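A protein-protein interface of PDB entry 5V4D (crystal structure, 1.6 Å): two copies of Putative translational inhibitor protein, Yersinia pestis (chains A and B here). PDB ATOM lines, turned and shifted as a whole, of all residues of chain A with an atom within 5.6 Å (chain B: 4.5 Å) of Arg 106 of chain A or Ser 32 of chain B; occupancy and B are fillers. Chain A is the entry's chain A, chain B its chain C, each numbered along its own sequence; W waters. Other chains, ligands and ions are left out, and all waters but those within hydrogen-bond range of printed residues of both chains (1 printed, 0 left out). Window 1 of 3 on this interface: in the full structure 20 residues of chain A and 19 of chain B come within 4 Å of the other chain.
The backbone carbonyl oxygen (O) of Pro 104 of chain A is in hydrogen-bond range of the backbone NH (N) of Ser 20 of chain B (3.1 Å). The backbone NH of Arg 106 of chain A sits at hydrogen-bond distance from the side-chain hydroxyl of Ser 32 of chain B, 2.8 Å away. O of Arg 106 of chain A is in hydrogen-bond range of N of Gly 33 of chain B (3.1 Å). OG of Ser 107 of chain A sits at hydrogen-bond distance from N of Gly 33 of chain B, at 3.0 Å.
The side-chain hydroxyl (OG1) of Thr 78 of chain A lies within hydrogen-bond range of the side-chain amino group (NZ) of Lys 76 of chain A (3.1 Å). OG1 of Thr 77 of chain A lies within hydrogen-bond range of OH of Tyr 94 of chain A (2.8 Å). The backbone carbonyl oxygen of Ala 105 of chain A sits at hydrogen-bond distance from the backbone NH of Thr 77 of chain A (2.9 Å). The backbone carbonyl oxygen (O) of Thr 77 of chain A lies within hydrogen-bond range of the backbone NH (N) of Ser 107 of chain A (3.1 Å). N of Ile 79 of chain A is in hydrogen-bond range of O of Ser 107 of chain A (2.8 Å). The side-chain amide oxygen (OD1) of Asn 91 of chain A lies within hydrogen-bond range of the guanidinium group (NH1) of Arg 106 of chain A (2.9 Å).
Among the printed residues, merely in contact across the chains: Ala 105 of chain A with Tyr 30 of chain B, Ala 105 of chain A with Ser 32 of chain B, Pro 104 of chain A with Tyr 19 of chain B, Tyr 94 of chain A with Pro 18 of chain B, Ala 105 of chain A with Ser 20 of chain B, Arg 106 of chain A with Tyr 19 of chain B, Lys 76 of chain A with Ala 31 of chain B, Asn 91 of chain A with Pro 18 of chain B and Arg 106 of chain A with Pro 18 of chain B.
Of chain A, only Ala 105 and Arg 106 come within 4 Å of Ser 32 of chain B. Of the printed residues of chain B, Pro 104 of chain A touches Tyr 19 (3.4 Å) and Ser 20 (3.1 Å). Of the printed residues of chain B, Ser 107 of chain A touches Gly 33. Printed residues of chain B within 4 Å of Tyr 94 of chain A: Pro 18. Ile 79 of chain A touches none of the printed residues of chain B. Gly 17 of chain B touches none of the printed residues of chain A. The nearest printed residue of chain B that does not touch Arg 106 of chain A is Gly 17 of chain B (4.05 Å). The nearest residue of chain A that does not touch Ser 32 of chain B is Ser 107 of chain A (4.1 Å).
Hydrophobic or aromatic side chains of chain B within 4 Å of the printed part of chain A: Pro 18 and Tyr 19. Of the 11 printed residues of chain A, 7 touch a printed residue of chain B. Hydrophobic or aromatic side chains of chain A that line the printed part of chain B: Tyr 94 and Ala 105. Among the printed residues, 13 pairs touch across the chains. Among the printed residues, no Asp or Glu carboxylate lies within 4 Å of a Lys or Arg side-chain nitrogen of the other chain.
No position is printed for both chains.
Water W1 lies within hydrogen-bond range of OH of Tyr 94 of chain A (2.6 Å), O of Pro 104 of chain A (2.7 Å) and O of Pro 18 of chain B (2.8 Å).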
ATOM      1  N   LYS A  76      15.358 -22.832  27.685  1.00  0.00           N
ATOM      2  CA  LYS A  76      14.624 -24.007  27.228  1.00  0.00           C
ATOM      3  C   LYS A  76      15.476 -25.236  27.511  1.00  0.00           C
ATOM      4  O   LYS A  76      16.697 -25.180  27.341  1.00  0.00           O
ATOM      5  CB  LYS A  76      14.329 -23.886  25.719  1.00  0.00           C
ATOM      6  CG  LYS A  76      13.843 -25.184  25.001  1.00  0.00           C
ATOM      7  CD  LYS A  76      12.450 -25.577  25.502  1.00  0.00           C
ATOM      8  CE  LYS A  76      11.766 -26.686  24.603  1.00  0.00           C
ATOM      9  NZ  LYS A  76      12.683 -27.862  24.522  1.00  0.00           N
ATOM     10  N   THR A  77      14.843 -26.313  27.992  1.00  0.00           N
ATOM     11  CA  THR A  77      15.514 -27.580  28.226  1.00  0.00           C
ATOM     12  C   THR A  77      14.694 -28.696  27.589  1.00  0.00           C
ATOM     13  O   THR A  77      13.492 -28.532  27.334  1.00  0.00           O
ATOM     14  CB  THR A  77      15.698 -27.908  29.723  1.00  0.00           C
ATOM     15  OG1 THR A  77      14.412 -28.227  30.296  1.00  0.00           O
ATOM     16  CG2 THR A  77      16.277 -26.737  30.486  1.00  0.00           C
ATOM     17  N   THR A  78      15.343 -29.830  27.335  1.00  0.00           N
ATOM     18  CA  THR A  78      14.648 -31.073  26.994  1.00  0.00           C
ATOM     19  C   THR A  78      15.140 -32.151  27.941  1.00  0.00           C
ATOM     20  O   THR A  78      16.352 -32.300  28.145  1.00  0.00           O
ATOM     21  CB  THR A  78      14.918 -31.492  25.537  1.00  0.00           C
ATOM     22  OG1 THR A  78      14.470 -30.439  24.685  1.00  0.00           O
ATOM     23  CG2 THR A  78      14.206 -32.780  25.165  1.00  0.00           C
ATOM     24  N   ILE A  79      14.207 -32.866  28.540  1.00  0.00           N
ATOM     25  CA  ILE A  79      14.525 -34.011  29.380  1.00  0.00           C
ATOM     26  C   ILE A  79      14.237 -35.284  28.590  1.00  0.00           C
ATOM     27  O   ILE A  79      13.081 -35.547  28.229  1.00  0.00           O
ATOM     28  CB  ILE A  79      13.700 -33.968  30.675  1.00  0.00           C
ATOM     29  CG1 ILE A  79      14.038 -32.701  31.463  1.00  0.00           C
ATOM     30  CG2 ILE A  79      13.966 -35.246  31.544  1.00  0.00           C
ATOM     31  CD1 ILE A  79      13.173 -32.548  32.751  1.00  0.00           C
ATOM     32  N   ASN A  91      11.647 -34.294  38.318  1.00  0.00           N
ATOM     33  CA  ASN A  91      11.068 -32.960  38.551  1.00  0.00           C
ATOM     34  C   ASN A  91      11.361 -32.460  39.956  1.00  0.00           C
ATOM     35  O   ASN A  91      11.616 -31.262  40.157  1.00  0.00           O
ATOM     36  CB  ASN A  91       9.542 -33.001  38.329  1.00  0.00           C
ATOM     37  CG  ASN A  91       9.169 -33.051  36.873  1.00  0.00           C
ATOM     38  OD1 ASN A  91       9.936 -32.620  36.043  1.00  0.00           O
ATOM     39  ND2 ASN A  91       7.978 -33.578  36.559  1.00  0.00           N
ATOM     40  N   TYR A  94      15.003 -31.308  39.844  1.00  0.00           N
ATOM     41  CA  TYR A  94      15.129 -30.237  38.870  1.00  0.00           C
ATOM     42  C   TYR A  94      14.550 -28.937  39.404  1.00  0.00           C
ATOM     43  O   TYR A  94      15.126 -27.857  39.214  1.00  0.00           O
ATOM     44  CB  TYR A  94      14.424 -30.703  37.600  1.00  0.00           C
ATOM     45  CG  TYR A  94      14.370 -29.807  36.392  1.00  0.00           C
ATOM     46  CD1 TYR A  94      15.127 -30.123  35.261  1.00  0.00           C
ATOM     47  CD2 TYR A  94      13.462 -28.742  36.327  1.00  0.00           C
ATOM     48  CE1 TYR A  94      15.034 -29.348  34.120  1.00  0.00           C
ATOM     49  CE2 TYR A  94      13.375 -27.964  35.194  1.00  0.00           C
ATOM     50  CZ  TYR A  94      14.154 -28.284  34.100  1.00  0.00           C
ATOM     51  OH  TYR A  94      14.062 -27.494  32.967  1.00  0.00           O
ATOM     52  N   PRO A 104      12.635 -22.464  32.969  1.00  0.00           N
ATOM     53  CA  PRO A 104      12.754 -22.566  31.514  1.00  0.00           C
ATOM     54  C   PRO A 104      11.520 -23.214  30.897  1.00  0.00           C
ATOM     55  O   PRO A 104      10.803 -23.995  31.536  1.00  0.00           O
ATOM     56  CB  PRO A 104      13.986 -23.461  31.336  1.00  0.00           C
ATOM     57  CG  PRO A 104      14.797 -23.239  32.600  1.00  0.00           C
ATOM     58  CD  PRO A 104      13.747 -23.132  33.681  1.00  0.00           C
ATOM     59  N   ALA A 105      11.301 -22.916  29.617  1.00  0.00           N
ATOM     60  CA  ALA A 105      10.433 -23.782  28.807  1.00  0.00           C
ATOM     61  C   ALA A 105      11.045 -25.189  28.735  1.00  0.00           C
ATOM     62  O   ALA A 105      12.235 -25.380  28.975  1.00  0.00           O
ATOM     63  CB  ALA A 105      10.269 -23.196  27.405  1.00  0.00           C
ATOM     64  N   ARG A 106      10.216 -26.195  28.412  1.00  0.00           N
ATOM     65  CA  ARG A 106      10.699 -27.572  28.600  1.00  0.00           C
ATOM     66  C   ARG A 106       9.893 -28.532  27.751  1.00  0.00           C
ATOM     67  O   ARG A 106       8.727 -28.285  27.465  1.00  0.00           O
ATOM     68  CB  ARG A 106      10.578 -27.997  30.062  1.00  0.00           C
ATOM     69  CG  ARG A 106      11.432 -29.222  30.347  1.00  0.00           C
ATOM     70  CD  ARG A 106      11.432 -29.437  31.846  1.00  0.00           C
ATOM     71  NE  ARG A 106      10.133 -29.991  32.225  1.00  0.00           N
ATOM     72  CZ  ARG A 106       9.843 -30.454  33.429  1.00  0.00           C
ATOM     73  NH1 ARG A 106      10.762 -30.405  34.402  1.00  0.00           N
ATOM     74  NH2 ARG A 106       8.632 -30.949  33.645  1.00  0.00           N
ATOM     75  N   SER A 107      10.547 -29.598  27.295  1.00  0.00           N
ATOM     76  CA  SER A 107       9.845 -30.798  26.832  1.00  0.00           C
ATOM     77  C   SER A 107      10.435 -32.007  27.538  1.00  0.00           C
ATOM     78  O   SER A 107      11.637 -32.046  27.789  1.00  0.00           O
ATOM     79  CB  SER A 107       9.985 -30.972  25.319  1.00  0.00           C
ATOM     80  OG  SER A 107       9.364 -29.849  24.656  1.00  0.00           O
ATOM     81  N   THR A 108       9.604 -33.036  27.749  1.00  0.00           N
ATOM     82  CA  THR A 108      10.001 -34.284  28.395  1.00  0.00           C
ATOM     83  C   THR A 108       9.475 -35.411  27.532  1.00  0.00           C
ATOM     84  O   THR A 108       8.284 -35.424  27.196  1.00  0.00           O
ATOM     85  CB  THR A 108       9.402 -34.422  29.807  1.00  0.00           C
ATOM     86  OG1 THR A 108       9.845 -33.329  30.616  1.00  0.00           O
ATOM     87  CG2 THR A 108       9.857 -35.794  30.447  1.00  0.00           C
ATOM     88  N   GLY B  17       4.785 -29.393  36.375  1.00  0.00           N
ATOM     89  CA  GLY B  17       6.205 -29.529  36.556  1.00  0.00           C
ATOM     90  C   GLY B  17       6.831 -28.156  36.568  1.00  0.00           C
ATOM     91  O   GLY B  17       6.189 -27.156  36.211  1.00  0.00           O
ATOM     92  N   PRO B  18       8.058 -28.081  37.000  1.00  0.00           N
ATOM     93  CA  PRO B  18       8.805 -26.809  37.166  1.00  0.00           C
ATOM     94  C   PRO B  18       9.282 -26.243  35.835  1.00  0.00           C
ATOM     95  O   PRO B  18      10.477 -26.211  35.506  1.00  0.00           O
ATOM     96  CB  PRO B  18       9.962 -27.219  38.080  1.00  0.00           C
ATOM     97  CG  PRO B  18      10.152 -28.676  37.821  1.00  0.00           C
ATOM     98  CD  PRO B  18       8.784 -29.231  37.578  1.00  0.00           C
ATOM     99  N   TYR B  19       8.317 -25.751  35.067  1.00  0.00           N
ATOM    100  CA  TYR B  19       8.559 -25.228  33.727  1.00  0.00           C
ATOM    101  C   TYR B  19       7.564 -24.132  33.409  1.00  0.00           C
ATOM    102  O   TYR B  19       6.526 -23.995  34.071  1.00  0.00           O
ATOM    103  CB  TYR B  19       8.498 -26.347  32.658  1.00  0.00           C
ATOM    104  CG  TYR B  19       7.170 -26.942  32.405  1.00  0.00           C
ATOM    105  CD1 TYR B  19       6.448 -26.566  31.301  1.00  0.00           C
ATOM    106  CD2 TYR B  19       6.665 -27.922  33.238  1.00  0.00           C
ATOM    107  CE1 TYR B  19       5.219 -27.128  31.018  1.00  0.00           C
ATOM    108  CE2 TYR B  19       5.399 -28.477  32.974  1.00  0.00           C
ATOM    109  CZ  TYR B  19       4.700 -28.059  31.869  1.00  0.00           C
ATOM    110  OH  TYR B  19       3.468 -28.616  31.587  1.00  0.00           O
ATOM    111  N   SER B  20       7.895 -23.329  32.401  1.00  0.00           N
ATOM    112  CA  SER B  20       7.019 -22.254  31.952  1.00  0.00           C
ATOM    113  C   SER B  20       6.391 -22.659  30.629  1.00  0.00           C
ATOM    114  O   SER B  20       7.011 -23.379  29.856  1.00  0.00           O
ATOM    115  CB  SER B  20       7.792 -20.936  31.762  1.00  0.00           C
ATOM    116  OG  SER B  20       8.312 -20.447  33.007  1.00  0.00           O
ATOM    117  N   GLN B  21       5.164 -22.177  30.356  1.00  0.00           N
ATOM    118  CA  GLN B  21       4.524 -22.489  29.064  1.00  0.00           C
ATOM    119  C   GLN B  21       5.400 -22.086  27.878  1.00  0.00           C
ATOM    120  O   GLN B  21       5.554 -22.853  26.929  1.00  0.00           O
ATOM    121  CB  GLN B  21       3.153 -21.813  28.957  1.00  0.00           C
ATOM    122  CG  GLN B  21       2.130 -22.392  29.933  1.00  0.00           C
ATOM    123  CD  GLN B  21       0.867 -21.575  29.884  1.00  0.00           C
ATOM    124  OE1 GLN B  21       0.902 -20.412  29.497  1.00  0.00           O
ATOM    125  NE2 GLN B  21      -0.272 -22.184  30.254  1.00  0.00           N
ATOM    126  N   ALA B  22       6.030 -20.920  27.938  1.00  0.00           N
ATOM    127  CA  ALA B  22       7.027 -20.553  26.942  1.00  0.00           C
ATOM    128  C   ALA B  22       7.919 -19.477  27.540  1.00  0.00           C
ATOM    129  O   ALA B  22       7.552 -18.827  28.524  1.00  0.00           O
ATOM    130  CB  ALA B  22       6.376 -20.045  25.652  1.00  0.00           C
ATOM    131  N   TYR B  30      10.423 -19.671  22.675  1.00  0.00           N
ATOM    132  CA  TYR B  30      10.690 -21.090  22.891  1.00  0.00           C
ATOM    133  C   TYR B  30       9.501 -21.639  23.649  1.00  0.00           C
ATOM    134  O   TYR B  30       9.347 -21.388  24.855  1.00  0.00           O
ATOM    135  CB  TYR B  30      11.996 -21.297  23.667  1.00  0.00           C
ATOM    136  CG  TYR B  30      13.177 -20.736  22.930  1.00  0.00           C
ATOM    137  CD1 TYR B  30      13.916 -21.535  22.051  1.00  0.00           C
ATOM    138  CD2 TYR B  30      13.541 -19.378  23.074  1.00  0.00           C
ATOM    139  CE1 TYR B  30      14.999 -21.007  21.334  1.00  0.00           C
ATOM    140  CE2 TYR B  30      14.638 -18.875  22.403  1.00  0.00           C
ATOM    141  CZ  TYR B  30      15.352 -19.683  21.531  1.00  0.00           C
ATOM    142  OH  TYR B  30      16.424 -19.138  20.842  1.00  0.00           O
ATOM    143  N   ALA B  31       8.623 -22.366  22.948  1.00  0.00           N
ATOM    144  CA  ALA B  31       7.467 -22.963  23.601  1.00  0.00           C
ATOM    145  C   ALA B  31       7.807 -24.327  24.215  1.00  0.00           C
ATOM    146  O   ALA B  31       8.555 -25.125  23.627  1.00  0.00           O
ATOM    147  CB  ALA B  31       6.327 -23.140  22.602  1.00  0.00           C
ATOM    148  N   SER B  32       7.235 -24.599  25.395  1.00  0.00           N
ATOM    149  CA  SER B  32       7.288 -25.961  25.935  1.00  0.00           C
ATOM    150  C   SER B  32       6.508 -26.900  25.032  1.00  0.00           C
ATOM    151  O   SER B  32       5.569 -26.493  24.366  1.00  0.00           O
ATOM    152  CB  SER B  32       6.710 -26.015  27.358  1.00  0.00           C
ATOM    153  OG  SER B  32       7.562 -25.258  28.222  1.00  0.00           O
ATOM    154  N   GLY B  33       6.929 -28.161  24.988  1.00  0.00           N
ATOM    155  CA  GLY B  33       6.141 -29.144  24.250  1.00  0.00           C
ATOM    156  C   GLY B  33       4.731 -29.175  24.788  1.00  0.00           C
ATOM    157  O   GLY B  33       4.518 -29.221  26.013  1.00  0.00           O
ATOM    158  N   GLN B  34       3.752 -29.122  23.888  1.00  0.00           N
ATOM    159  CA  GLN B  34       2.358 -29.147  24.284  1.00  0.00           C
ATOM    160  C   GLN B  34       1.823 -30.547  24.119  1.00  0.00           C
ATOM    161  O   GLN B  34       2.087 -31.201  23.094  1.00  0.00           O
ATOM    162  CB  GLN B  34       1.530 -28.150  23.446  1.00  0.00           C
ATOM    163  CG  GLN B  34       1.676 -26.698  23.898  1.00  0.00           C
ATOM    164  CD  GLN B  34       1.100 -26.518  25.317  1.00  0.00           C
ATOM    165  OE1 GLN B  34       0.136 -27.200  25.707  1.00  0.00           O
ATOM    166  NE2 GLN B  34       1.741 -25.681  26.104  1.00  0.00           N
ATOM    167  N   ILE B 122       3.945 -31.695  20.745  1.00  0.00           N
ATOM    168  CA  ILE B 122       4.576 -30.882  19.706  1.00  0.00           C
ATOM    169  C   ILE B 122       5.248 -29.670  20.346  1.00  0.00           C
ATOM    170  O   ILE B 122       4.607 -28.939  21.117  1.00  0.00           O
ATOM    171  CB  ILE B 122       3.566 -30.454  18.621  1.00  0.00           C
ATOM    172  CG1 ILE B 122       2.952 -31.698  17.930  1.00  0.00           C
ATOM    173  CG2 ILE B 122       4.261 -29.486  17.575  1.00  0.00           C
ATOM    174  CD1 ILE B 122       1.989 -31.340  16.827  1.00  0.00           C
HETATM  175  O   HOH W   1      11.915 -25.977  33.070  1.00  0.00           O
